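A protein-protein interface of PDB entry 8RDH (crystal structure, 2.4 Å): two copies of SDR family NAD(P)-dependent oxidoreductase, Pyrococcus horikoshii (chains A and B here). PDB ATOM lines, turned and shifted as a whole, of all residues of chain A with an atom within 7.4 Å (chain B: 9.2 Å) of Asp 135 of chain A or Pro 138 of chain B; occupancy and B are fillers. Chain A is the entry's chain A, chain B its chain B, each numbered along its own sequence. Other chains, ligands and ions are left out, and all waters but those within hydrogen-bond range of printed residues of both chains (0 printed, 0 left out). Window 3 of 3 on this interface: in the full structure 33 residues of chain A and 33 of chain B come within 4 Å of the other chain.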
ATOM      1  N   TYR A 124      31.245  24.489  27.296  1.00  0.00           N
ATOM      2  CA  TYR A 124      30.264  24.602  28.366  1.00  0.00           C
ATOM      3  C   TYR A 124      30.918  24.837  29.721  1.00  0.00           C
ATOM      4  O   TYR A 124      30.231  25.242  30.665  1.00  0.00           O
ATOM      5  CB  TYR A 124      29.408  23.333  28.420  1.00  0.00           C
ATOM      6  CG  TYR A 124      28.626  23.055  27.152  1.00  0.00           C
ATOM      7  CD1 TYR A 124      27.655  23.939  26.700  1.00  0.00           C
ATOM      8  CD2 TYR A 124      28.864  21.909  26.405  1.00  0.00           C
ATOM      9  CE1 TYR A 124      26.938  23.686  25.547  1.00  0.00           C
ATOM     10  CE2 TYR A 124      28.155  21.648  25.249  1.00  0.00           C
ATOM     11  CZ  TYR A 124      27.192  22.540  24.825  1.00  0.00           C
ATOM     12  OH  TYR A 124      26.481  22.286  23.675  1.00  0.00           O
ATOM     13  N   THR A 132      24.242  18.074  29.278  1.00  0.00           N
ATOM     14  CA  THR A 132      24.308  19.469  28.843  1.00  0.00           C
ATOM     15  C   THR A 132      23.735  19.626  27.438  1.00  0.00           C
ATOM     16  O   THR A 132      24.226  18.978  26.508  1.00  0.00           O
ATOM     17  CB  THR A 132      25.750  19.957  28.864  1.00  0.00           C
ATOM     18  OG1 THR A 132      26.364  19.584  30.103  1.00  0.00           O
ATOM     19  CG2 THR A 132      25.809  21.469  28.715  1.00  0.00           C
ATOM     20  N   PRO A 133      22.726  20.473  27.235  1.00  0.00           N
ATOM     21  CA  PRO A 133      22.176  20.686  25.894  1.00  0.00           C
ATOM     22  C   PRO A 133      22.873  21.811  25.133  1.00  0.00           C
ATOM     23  O   PRO A 133      23.623  22.614  25.695  1.00  0.00           O
ATOM     24  CB  PRO A 133      20.718  21.050  26.191  1.00  0.00           C
ATOM     25  CG  PRO A 133      20.821  21.821  27.458  1.00  0.00           C
ATOM     26  CD  PRO A 133      21.902  21.135  28.263  1.00  0.00           C
ATOM     27  N   GLU A 134      22.583  21.864  23.828  1.00  0.00           N
ATOM     28  CA  GLU A 134      23.252  22.810  22.938  1.00  0.00           C
ATOM     29  C   GLU A 134      22.984  24.260  23.314  1.00  0.00           C
ATOM     30  O   GLU A 134      23.807  25.135  23.017  1.00  0.00           O
ATOM     31  CB  GLU A 134      22.810  22.581  21.491  1.00  0.00           C
ATOM     32  CG  GLU A 134      23.405  21.351  20.825  1.00  0.00           C
ATOM     33  CD  GLU A 134      22.653  20.070  21.144  1.00  0.00           C
ATOM     34  OE1 GLU A 134      21.739  20.100  21.995  1.00  0.00           O
ATOM     35  OE2 GLU A 134      22.983  19.028  20.541  1.00  0.00           O
ATOM     36  N   ASP A 135      21.845  24.547  23.942  1.00  0.00           N
ATOM     37  CA  ASP A 135      21.471  25.918  24.260  1.00  0.00           C
ATOM     38  C   ASP A 135      21.760  26.279  25.713  1.00  0.00           C
ATOM     39  O   ASP A 135      21.154  27.214  26.246  1.00  0.00           O
ATOM     40  CB  ASP A 135      19.997  26.159  23.941  1.00  0.00           C
ATOM     41  CG  ASP A 135      19.065  25.335  24.804  1.00  0.00           C
ATOM     42  OD1 ASP A 135      19.543  24.439  25.531  1.00  0.00           O
ATOM     43  OD2 ASP A 135      17.844  25.590  24.751  1.00  0.00           O
ATOM     44  N   TYR A 136      22.656  25.547  26.364  1.00  0.00           N
ATOM     45  CA  TYR A 136      23.064  25.883  27.720  1.00  0.00           C
ATOM     46  C   TYR A 136      23.900  27.159  27.730  1.00  0.00           C
ATOM     47  O   TYR A 136      24.729  27.387  26.845  1.00  0.00           O
ATOM     48  CB  TYR A 136      23.854  24.721  28.318  1.00  0.00           C
ATOM     49  CG  TYR A 136      24.488  25.014  29.651  1.00  0.00           C
ATOM     50  CD1 TYR A 136      25.753  25.581  29.726  1.00  0.00           C
ATOM     51  CD2 TYR A 136      23.833  24.712  30.834  1.00  0.00           C
ATOM     52  CE1 TYR A 136      26.344  25.848  30.941  1.00  0.00           C
ATOM     53  CE2 TYR A 136      24.415  24.978  32.058  1.00  0.00           C
ATOM     54  CZ  TYR A 136      25.673  25.546  32.104  1.00  0.00           C
ATOM     55  OH  TYR A 136      26.266  25.812  33.316  1.00  0.00           O
ATOM     56  N   ALA A 137      23.674  27.996  28.738  1.00  0.00           N
ATOM     57  CA  ALA A 137      24.382  29.262  28.869  1.00  0.00           C
ATOM     58  C   ALA A 137      24.197  29.773  30.290  1.00  0.00           C
ATOM     59  O   ALA A 137      23.326  29.285  31.019  1.00  0.00           O
ATOM     60  CB  ALA A 137      23.872  30.293  27.850  1.00  0.00           C
ATOM     61  N   PRO A 138      25.010  30.751  30.723  1.00  0.00           N
ATOM     62  CA  PRO A 138      26.147  31.362  30.012  1.00  0.00           C
ATOM     63  C   PRO A 138      27.285  30.377  29.774  1.00  0.00           C
ATOM     64  O   PRO A 138      27.605  29.562  30.634  1.00  0.00           O
ATOM     65  CB  PRO A 138      26.577  32.504  30.951  1.00  0.00           C
ATOM     66  CG  PRO A 138      25.371  32.788  31.798  1.00  0.00           C
ATOM     67  CD  PRO A 138      24.737  31.443  31.993  1.00  0.00           C
ATOM     68  N   LEU A 139      27.909  30.440  28.601  1.00  0.00           N
ATOM     69  CA  LEU A 139      29.068  29.611  28.299  1.00  0.00           C
ATOM     70  C   LEU A 139      30.301  30.199  28.975  1.00  0.00           C
ATOM     71  O   LEU A 139      30.691  31.337  28.691  1.00  0.00           O
ATOM     72  CB  LEU A 139      29.250  29.509  26.787  1.00  0.00           C
ATOM     73  CG  LEU A 139      28.163  28.640  26.150  1.00  0.00           C
ATOM     74  CD1 LEU A 139      27.864  29.053  24.725  1.00  0.00           C
ATOM     75  CD2 LEU A 139      28.582  27.178  26.203  1.00  0.00           C
ATOM     76  N   GLU A 153      34.094  29.055  17.261  1.00  0.00           N
ATOM     77  CA  GLU A 153      32.671  28.945  16.942  1.00  0.00           C
ATOM     78  C   GLU A 153      32.068  30.311  16.630  1.00  0.00           C
ATOM     79  O   GLU A 153      31.340  30.481  15.643  1.00  0.00           O
ATOM     80  CB  GLU A 153      31.906  28.315  18.107  1.00  0.00           C
ATOM     81  CG  GLU A 153      32.138  26.834  18.352  1.00  0.00           C
ATOM     82  CD  GLU A 153      31.171  26.282  19.396  1.00  0.00           C
ATOM     83  OE1 GLU A 153      30.353  27.066  19.922  1.00  0.00           O
ATOM     84  OE2 GLU A 153      31.211  25.068  19.683  1.00  0.00           O
ATOM     85  N   ARG A 171      29.848  19.991  18.649  1.00  0.00           N
ATOM     86  CA  ARG A 171      30.587  19.961  19.908  1.00  0.00           C
ATOM     87  C   ARG A 171      30.774  18.503  20.315  1.00  0.00           C
ATOM     88  O   ARG A 171      29.815  17.833  20.711  1.00  0.00           O
ATOM     89  CB  ARG A 171      29.851  20.747  20.989  1.00  0.00           C
ATOM     90  CG  ARG A 171      29.826  22.245  20.746  1.00  0.00           C
ATOM     91  CD  ARG A 171      28.732  22.909  21.555  1.00  0.00           C
ATOM     92  NE  ARG A 171      28.670  24.344  21.313  1.00  0.00           N
ATOM     93  CZ  ARG A 171      27.601  25.095  21.543  1.00  0.00           C
ATOM     94  NH1 ARG A 171      26.476  24.573  22.005  1.00  0.00           N
ATOM     95  NH2 ARG A 171      27.659  26.399  21.292  1.00  0.00           N
ATOM     96  N   ASP A 236      24.199  25.827  12.635  1.00  0.00           N
ATOM     97  CA  ASP A 236      23.543  24.839  13.477  1.00  0.00           C
ATOM     98  C   ASP A 236      24.539  24.264  14.472  1.00  0.00           C
ATOM     99  O   ASP A 236      25.735  24.158  14.193  1.00  0.00           O
ATOM    100  CB  ASP A 236      22.921  23.705  12.647  1.00  0.00           C
ATOM    101  CG  ASP A 236      21.574  23.246  13.195  1.00  0.00           C
ATOM    102  OD1 ASP A 236      21.171  23.722  14.281  1.00  0.00           O
ATOM    103  OD2 ASP A 236      20.919  22.405  12.539  1.00  0.00           O
ATOM    104  N   PHE A 237      24.012  23.861  15.628  1.00  0.00           N
ATOM    105  CA  PHE A 237      24.800  23.444  16.780  1.00  0.00           C
ATOM    106  C   PHE A 237      24.351  22.052  17.193  1.00  0.00           C
ATOM    107  O   PHE A 237      23.159  21.832  17.432  1.00  0.00           O
ATOM    108  CB  PHE A 237      24.622  24.426  17.946  1.00  0.00           C
ATOM    109  CG  PHE A 237      25.146  25.805  17.666  1.00  0.00           C
ATOM    110  CD1 PHE A 237      24.357  26.738  17.019  1.00  0.00           C
ATOM    111  CD2 PHE A 237      26.422  26.173  18.066  1.00  0.00           C
ATOM    112  CE1 PHE A 237      24.832  28.007  16.755  1.00  0.00           C
ATOM    113  CE2 PHE A 237      26.901  27.444  17.808  1.00  0.00           C
ATOM    114  CZ  PHE A 237      26.105  28.362  17.153  1.00  0.00           C
ATOM    115  N   ASN A 239      25.550  18.673  19.793  1.00  0.00           N
ATOM    116  CA  ASN A 239      26.413  17.876  20.651  1.00  0.00           C
ATOM    117  C   ASN A 239      26.604  16.500  20.027  1.00  0.00           C
ATOM    118  O   ASN A 239      25.684  15.944  19.419  1.00  0.00           O
ATOM    119  CB  ASN A 239      25.812  17.728  22.050  1.00  0.00           C
ATOM    120  CG  ASN A 239      25.791  19.034  22.831  1.00  0.00           C
ATOM    121  OD1 ASN A 239      26.663  19.887  22.668  1.00  0.00           O
ATOM    122  ND2 ASN A 239      24.795  19.186  23.703  1.00  0.00           N
ATOM    123  N   LYS A 290      19.250  16.173  20.150  1.00  0.00           N
ATOM    124  CA  LYS A 290      19.225  16.841  18.855  1.00  0.00           C
ATOM    125  C   LYS A 290      19.899  15.986  17.792  1.00  0.00           C
ATOM    126  O   LYS A 290      19.381  15.844  16.677  1.00  0.00           O
ATOM    127  CB  LYS A 290      19.902  18.202  18.979  1.00  0.00           C
ATOM    128  CG  LYS A 290      19.651  19.161  17.838  1.00  0.00           C
ATOM    129  CD  LYS A 290      20.327  20.492  18.146  1.00  0.00           C
ATOM    130  CE  LYS A 290      20.206  21.495  17.019  1.00  0.00           C
ATOM    131  NZ  LYS A 290      20.862  22.782  17.396  1.00  0.00           N
ATOM    132  N   THR B 122      25.322  42.341  20.504  1.00  0.00           N
ATOM    133  CA  THR B 122      25.469  41.633  19.240  1.00  0.00           C
ATOM    134  C   THR B 122      25.891  40.179  19.414  1.00  0.00           C
ATOM    135  O   THR B 122      25.777  39.403  18.461  1.00  0.00           O
ATOM    136  CB  THR B 122      26.491  42.358  18.363  1.00  0.00           C
ATOM    137  OG1 THR B 122      27.725  42.490  19.081  1.00  0.00           O
ATOM    138  CG2 THR B 122      25.983  43.728  17.974  1.00  0.00           C
ATOM    139  N   VAL B 123      26.376  39.790  20.596  1.00  0.00           N
ATOM    140  CA  VAL B 123      26.734  38.390  20.812  1.00  0.00           C
ATOM    141  C   VAL B 123      25.500  37.504  20.786  1.00  0.00           C
ATOM    142  O   VAL B 123      25.598  36.304  20.495  1.00  0.00           O
ATOM    143  CB  VAL B 123      27.490  38.211  22.140  1.00  0.00           C
ATOM    144  CG1 VAL B 123      28.705  39.124  22.185  1.00  0.00           C
ATOM    145  CG2 VAL B 123      26.566  38.463  23.337  1.00  0.00           C
ATOM    146  N   TYR B 124      24.328  38.065  21.097  1.00  0.00           N
ATOM    147  CA  TYR B 124      23.084  37.309  21.040  1.00  0.00           C
ATOM    148  C   TYR B 124      22.571  37.118  19.619  1.00  0.00           C
ATOM    149  O   TYR B 124      21.664  36.304  19.413  1.00  0.00           O
ATOM    150  CB  TYR B 124      22.005  37.999  21.878  1.00  0.00           C
ATOM    151  CG  TYR B 124      22.352  38.133  23.342  1.00  0.00           C
ATOM    152  CD1 TYR B 124      22.592  37.013  24.121  1.00  0.00           C
ATOM    153  CD2 TYR B 124      22.408  39.378  23.952  1.00  0.00           C
ATOM    154  CE1 TYR B 124      22.901  37.125  25.458  1.00  0.00           C
ATOM    155  CE2 TYR B 124      22.715  39.501  25.293  1.00  0.00           C
ATOM    156  CZ  TYR B 124      22.957  38.367  26.041  1.00  0.00           C
ATOM    157  OH  TYR B 124      23.265  38.465  27.376  1.00  0.00           O
ATOM    158  N   GLY B 125      23.107  37.857  18.646  1.00  0.00           N
ATOM    159  CA  GLY B 125      22.645  37.739  17.275  1.00  0.00           C
ATOM    160  C   GLY B 125      21.245  38.307  17.096  1.00  0.00           C
ATOM    161  O   GLY B 125      20.827  39.245  17.781  1.00  0.00           O
ATOM    162  N   ASP B 126      20.509  37.724  16.151  1.00  0.00           N
ATOM    163  CA  ASP B 126      19.090  38.034  15.988  1.00  0.00           C
ATOM    164  C   ASP B 126      18.348  37.206  17.025  1.00  0.00           C
ATOM    165  O   ASP B 126      17.881  36.098  16.755  1.00  0.00           O
ATOM    166  CB  ASP B 126      18.613  37.732  14.575  1.00  0.00           C
ATOM    167  CG  ASP B 126      19.017  38.803  13.577  1.00  0.00           C
ATOM    168  OD1 ASP B 126      18.898  40.003  13.902  1.00  0.00           O
ATOM    169  OD2 ASP B 126      19.437  38.446  12.458  1.00  0.00           O
ATOM    170  N   ALA B 127      18.242  37.751  18.233  1.00  0.00           N
ATOM    171  CA  ALA B 127      17.722  36.976  19.347  1.00  0.00           C
ATOM    172  C   ALA B 127      16.237  36.712  19.155  1.00  0.00           C
ATOM    173  O   ALA B 127      15.478  37.593  18.740  1.00  0.00           O
ATOM    174  CB  ALA B 127      17.956  37.710  20.667  1.00  0.00           C
ATOM    175  N   LYS B 128      15.829  35.486  19.459  1.00  0.00           N
ATOM    176  CA  LYS B 128      14.438  35.076  19.361  1.00  0.00           C
ATOM    177  C   LYS B 128      13.692  35.225  20.682  1.00  0.00           C
ATOM    178  O   LYS B 128      12.463  35.100  20.698  1.00  0.00           O
ATOM    179  CB  LYS B 128      14.365  33.635  18.850  1.00  0.00           C
ATOM    180  CG  LYS B 128      14.931  33.466  17.429  1.00  0.00           C
ATOM    181  CD  LYS B 128      13.881  33.835  16.371  1.00  0.00           C
ATOM    182  CE  LYS B 128      14.368  33.631  14.933  1.00  0.00           C
ATOM    183  NZ  LYS B 128      15.381  34.633  14.486  1.00  0.00           N
ATOM    184  N   VAL B 129      14.407  35.470  21.778  1.00  0.00           N
ATOM    185  CA  VAL B 129      13.821  35.741  23.087  1.00  0.00           C
ATOM    186  C   VAL B 129      14.108  37.200  23.423  1.00  0.00           C
ATOM    187  O   VAL B 129      15.269  37.588  23.612  1.00  0.00           O
ATOM    188  CB  VAL B 129      14.383  34.801  24.163  1.00  0.00           C
ATOM    189  CG1 VAL B 129      13.829  35.157  25.527  1.00  0.00           C
ATOM    190  CG2 VAL B 129      14.066  33.358  23.818  1.00  0.00           C
ATOM    191  N   THR B 132      16.152  39.899  26.007  1.00  0.00           N
ATOM    192  CA  THR B 132      17.137  38.832  25.930  1.00  0.00           C
ATOM    193  C   THR B 132      17.840  38.673  27.273  1.00  0.00           C
ATOM    194  O   THR B 132      18.418  39.643  27.774  1.00  0.00           O
ATOM    195  CB  THR B 132      18.149  39.149  24.837  1.00  0.00           C
ATOM    196  OG1 THR B 132      17.451  39.558  23.653  1.00  0.00           O
ATOM    197  CG2 THR B 132      19.003  37.937  24.521  1.00  0.00           C
ATOM    198  N   GLU B 134      20.694  36.928  30.095  1.00  0.00           N
ATOM    199  CA  GLU B 134      22.112  36.589  30.063  1.00  0.00           C
ATOM    200  C   GLU B 134      22.352  35.139  29.662  1.00  0.00           C
ATOM    201  O   GLU B 134      23.427  34.820  29.145  1.00  0.00           O
ATOM    202  CB  GLU B 134      22.753  36.860  31.424  1.00  0.00           C
ATOM    203  CG  GLU B 134      22.985  38.332  31.729  1.00  0.00           C
ATOM    204  CD  GLU B 134      21.745  39.017  32.264  1.00  0.00           C
ATOM    205  OE1 GLU B 134      20.666  38.387  32.265  1.00  0.00           O
ATOM    206  OE2 GLU B 134      21.853  40.184  32.694  1.00  0.00           O
ATOM    207  N   ASP B 135      21.384  34.250  29.889  1.00  0.00           N
ATOM    208  CA  ASP B 135      21.561  32.831  29.612  1.00  0.00           C
ATOM    209  C   ASP B 135      20.933  32.406  28.289  1.00  0.00           C
ATOM    210  O   ASP B 135      20.676  31.214  28.090  1.00  0.00           O
ATOM    211  CB  ASP B 135      20.977  32.002  30.754  1.00  0.00           C
ATOM    212  CG  ASP B 135      19.484  32.186  30.891  1.00  0.00           C
ATOM    213  OD1 ASP B 135      18.942  33.096  30.227  1.00  0.00           O
ATOM    214  OD2 ASP B 135      18.853  31.426  31.653  1.00  0.00           O
ATOM    215  N   TYR B 136      20.685  33.346  27.381  1.00  0.00           N
ATOM    216  CA  TYR B 136      20.160  32.992  26.070  1.00  0.00           C
ATOM    217  C   TYR B 136      21.234  32.277  25.261  1.00  0.00           C
ATOM    218  O   TYR B 136      22.407  32.661  25.278  1.00  0.00           O
ATOM    219  CB  TYR B 136      19.678  34.244  25.340  1.00  0.00           C
ATOM    220  CG  TYR B 136      19.243  34.009  23.912  1.00  0.00           C
ATOM    221  CD1 TYR B 136      17.943  33.623  23.617  1.00  0.00           C
ATOM    222  CD2 TYR B 136      20.129  34.182  22.857  1.00  0.00           C
ATOM    223  CE1 TYR B 136      17.539  33.407  22.311  1.00  0.00           C
ATOM    224  CE2 TYR B 136      19.735  33.969  21.550  1.00  0.00           C
ATOM    225  CZ  TYR B 136      18.438  33.580  21.283  1.00  0.00           C
ATOM    226  OH  TYR B 136      18.033  33.365  19.985  1.00  0.00           O
ATOM    227  N   ALA B 137      20.830  31.230  24.551  1.00  0.00           N
ATOM    228  CA  ALA B 137      21.753  30.432  23.758  1.00  0.00           C
ATOM    229  C   ALA B 137      20.943  29.583  22.790  1.00  0.00           C
ATOM    230  O   ALA B 137      19.726  29.435  22.959  1.00  0.00           O
ATOM    231  CB  ALA B 137      22.635  29.550  24.658  1.00  0.00           C
ATOM    232  N   PRO B 138      21.584  29.016  21.755  1.00  0.00           N
ATOM    233  CA  PRO B 138      22.996  29.164  21.368  1.00  0.00           C
ATOM    234  C   PRO B 138      23.326  30.590  20.939  1.00  0.00           C
ATOM    235  O   PRO B 138      22.512  31.262  20.308  1.00  0.00           O
ATOM    236  CB  PRO B 138      23.147  28.170  20.200  1.00  0.00           C
ATOM    237  CG  PRO B 138      22.015  27.195  20.366  1.00  0.00           C
ATOM    238  CD  PRO B 138      20.893  28.031  20.905  1.00  0.00           C
ATOM    239  N   LEU B 139      24.508  31.089  21.288  1.00  0.00           N
ATOM    240  CA  LEU B 139      24.938  32.403  20.830  1.00  0.00           C
ATOM    241  C   LEU B 139      25.360  32.291  19.374  1.00  0.00           C
ATOM    242  O   LEU B 139      26.275  31.527  19.041  1.00  0.00           O
ATOM    243  CB  LEU B 139      26.072  32.933  21.701  1.00  0.00           C
ATOM    244  CG  LEU B 139      25.601  33.336  23.098  1.00  0.00           C
ATOM    245  CD1 LEU B 139      26.713  33.203  24.116  1.00  0.00           C
ATOM    246  CD2 LEU B 139      25.060  34.753  23.065  1.00  0.00           C
ATOM    247  N   GLU B 140      24.684  33.039  18.509  1.00  0.00           N
ATOM    248  CA  GLU B 140      24.826  32.923  17.059  1.00  0.00           C
ATOM    249  C   GLU B 140      24.989  34.322  16.483  1.00  0.00           C
ATOM    250  O   GLU B 140      24.097  34.837  15.797  1.00  0.00           O
ATOM    251  CB  GLU B 140      23.618  32.210  16.449  1.00  0.00           C
ATOM    252  CG  GLU B 140      23.725  31.940  14.957  1.00  0.00           C
ATOM    253  CD  GLU B 140      22.499  31.228  14.405  1.00  0.00           C
ATOM    254  OE1 GLU B 140      21.782  30.574  15.192  1.00  0.00           O
ATOM    255  OE2 GLU B 140      22.257  31.321  13.182  1.00  0.00           O
ATOM    256  N   PRO B 141      26.113  34.978  16.767  1.00  0.00           N
ATOM    257  CA  PRO B 141      26.339  36.319  16.217  1.00  0.00           C
ATOM    258  C   PRO B 141      26.252  36.308  14.699  1.00  0.00           C
ATOM    259  O   PRO B 141      26.697  35.365  14.042  1.00  0.00           O
ATOM    260  CB  PRO B 141      27.749  36.679  16.707  1.00  0.00           C
ATOM    261  CG  PRO B 141      28.353  35.396  17.200  1.00  0.00           C
ATOM    262  CD  PRO B 141      27.206  34.553  17.658  1.00  0.00           C
ATOM    263  N   LEU B 150      32.143  38.091  21.125  1.00  0.00           N
ATOM    264  CA  LEU B 150      31.924  36.818  21.800  1.00  0.00           C
ATOM    265  C   LEU B 150      33.241  36.069  21.986  1.00  0.00           C
ATOM    266  O   LEU B 150      33.486  35.473  23.046  1.00  0.00           O
ATOM    267  CB  LEU B 150      30.920  35.986  21.005  1.00  0.00           C
ATOM    268  CG  LEU B 150      30.464  34.663  21.613  1.00  0.00           C
ATOM    269  CD1 LEU B 150      30.010  34.867  23.040  1.00  0.00           C
ATOM    270  CD2 LEU B 150      29.351  34.057  20.771  1.00  0.00           C
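The guanidinium group (NH1) of Arg 171 of chain A is in hydrogen-bond range of the backbone carbonyl oxygen (O) of Glu 134 of chain A, at 2.9 Å. The backbone NH (N) of Asn 239 of chain A is in hydrogen-bond range of the side-chain carboxylate (OE2) of Glu 134 of chain A (2.7 Å). NZ of Lys 290 of chain A sits at hydrogen-bond distance from O of Phe 237 of chain A (2.5 Å). OH of Tyr 136 of chain B sits at hydrogen-bond distance from N of Lys 128 of chain B (3.1 Å).
Pro 138 of chain B touches Glu 134 of chain A (CG to O, 3.8 Å). O of Asp 135 of chain A touches CB of Ala 137 of chain B, at 3.2 Å. O of Tyr 136 of chain A touches CB of Ala 137 of chain B (3.7 Å). O of Asp 135 of chain B touches CB of Ala 137 of chain A (3.3 Å). CB of Ala 137 of chain A touches O of Tyr 136 of chain B, 3.8 Å away. CB of Ala 137 of chain B touches CB of Ala 137 of chain A, 3.5 Å away. O of Glu 134 of chain B touches CG of Pro 138 of chain A, at 3.9 Å. Asp 135 of chain B touches Pro 138 of chain A (CB to CD, 3.998 Å). Phe 237 of chain A touches Pro 138 of chain B (CD1 to CB, 3.7 Å). Leu 139 of chain B touches Phe 237 of chain A (O to CZ, 3.7 Å).
Pro 133 of chain A touches none of the printed residues of chain B. Of the printed residues of chain B, Asp 135 of chain A touches Ala 137 and Pro 138. Printed residues of chain B within 4 Å of Ala 137 of chain A: Asp 135 (3.3 Å), Tyr 136 (3.8 Å) and Ala 137 (3.5 Å). Printed residues of chain B within 4 Å of Pro 138 of chain A: Glu 134 and Asp 135. Printed residues of chain A within 4 Å of Glu 134 of chain B: Pro 138 (3.9 Å). Of the printed residues of chain A, Asp 135 of chain B touches Ala 137 and Pro 138. Of chain A, only Glu 134, Asp 135 and Phe 237 come within 4 Å of Pro 138 of chain B. The nearest residue of chain A that does not touch Pro 138 of chain B is Arg 171 of chain A (5.0 Å).
Of the 18 printed residues of chain B, 6 touch a printed residue of chain A. Printed residues of chain B that touch a printed residue of chain A: Glu 134, Asp 135, Tyr 136, Ala 137, Pro 138 and Leu 139. Hydrophobic or aromatic side chains of chain B that line the printed part of chain A: Ala 137 and Pro 138. Of the 15 printed residues of chain A, 6 touch a printed residue of chain B. Printed residues of chain A that touch a printed residue of chain B: Glu 134, Asp 135, Tyr 136, Ala 137, Pro 138 and Phe 237. Hydrophobic or aromatic side chains of chain A within 4 Å of the printed part of chain B: Ala 137, Pro 138 and Phe 237. Among the printed residues, 11 pairs touch across the chains. Among the printed residues, no Asp or Glu carboxylate lies within 4 Å of a Lys or Arg side-chain nitrogen of the other chain.
Glu 134 of chain A touches Pro 138 of chain B, and with the chains exchanged Pro 138 of chain A touches Glu 134 of chain B. Asp 135 of chain A touches Ala 137 of chain B, and with the chains exchanged Ala 137 of chain A touches Asp 135 of chain B. Asp 135 of chain A touches Pro 138 of chain B, and with the chains exchanged Pro 138 of chain A touches Asp 135 of chain B. Tyr 136 of chain A touches Ala 137 of chain B, and with the chains exchanged Ala 137 of chain A touches Tyr 136 of chain B. Positions printed for both chains: 124, 132, 134, 135, 136, 137, 138 and 139.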
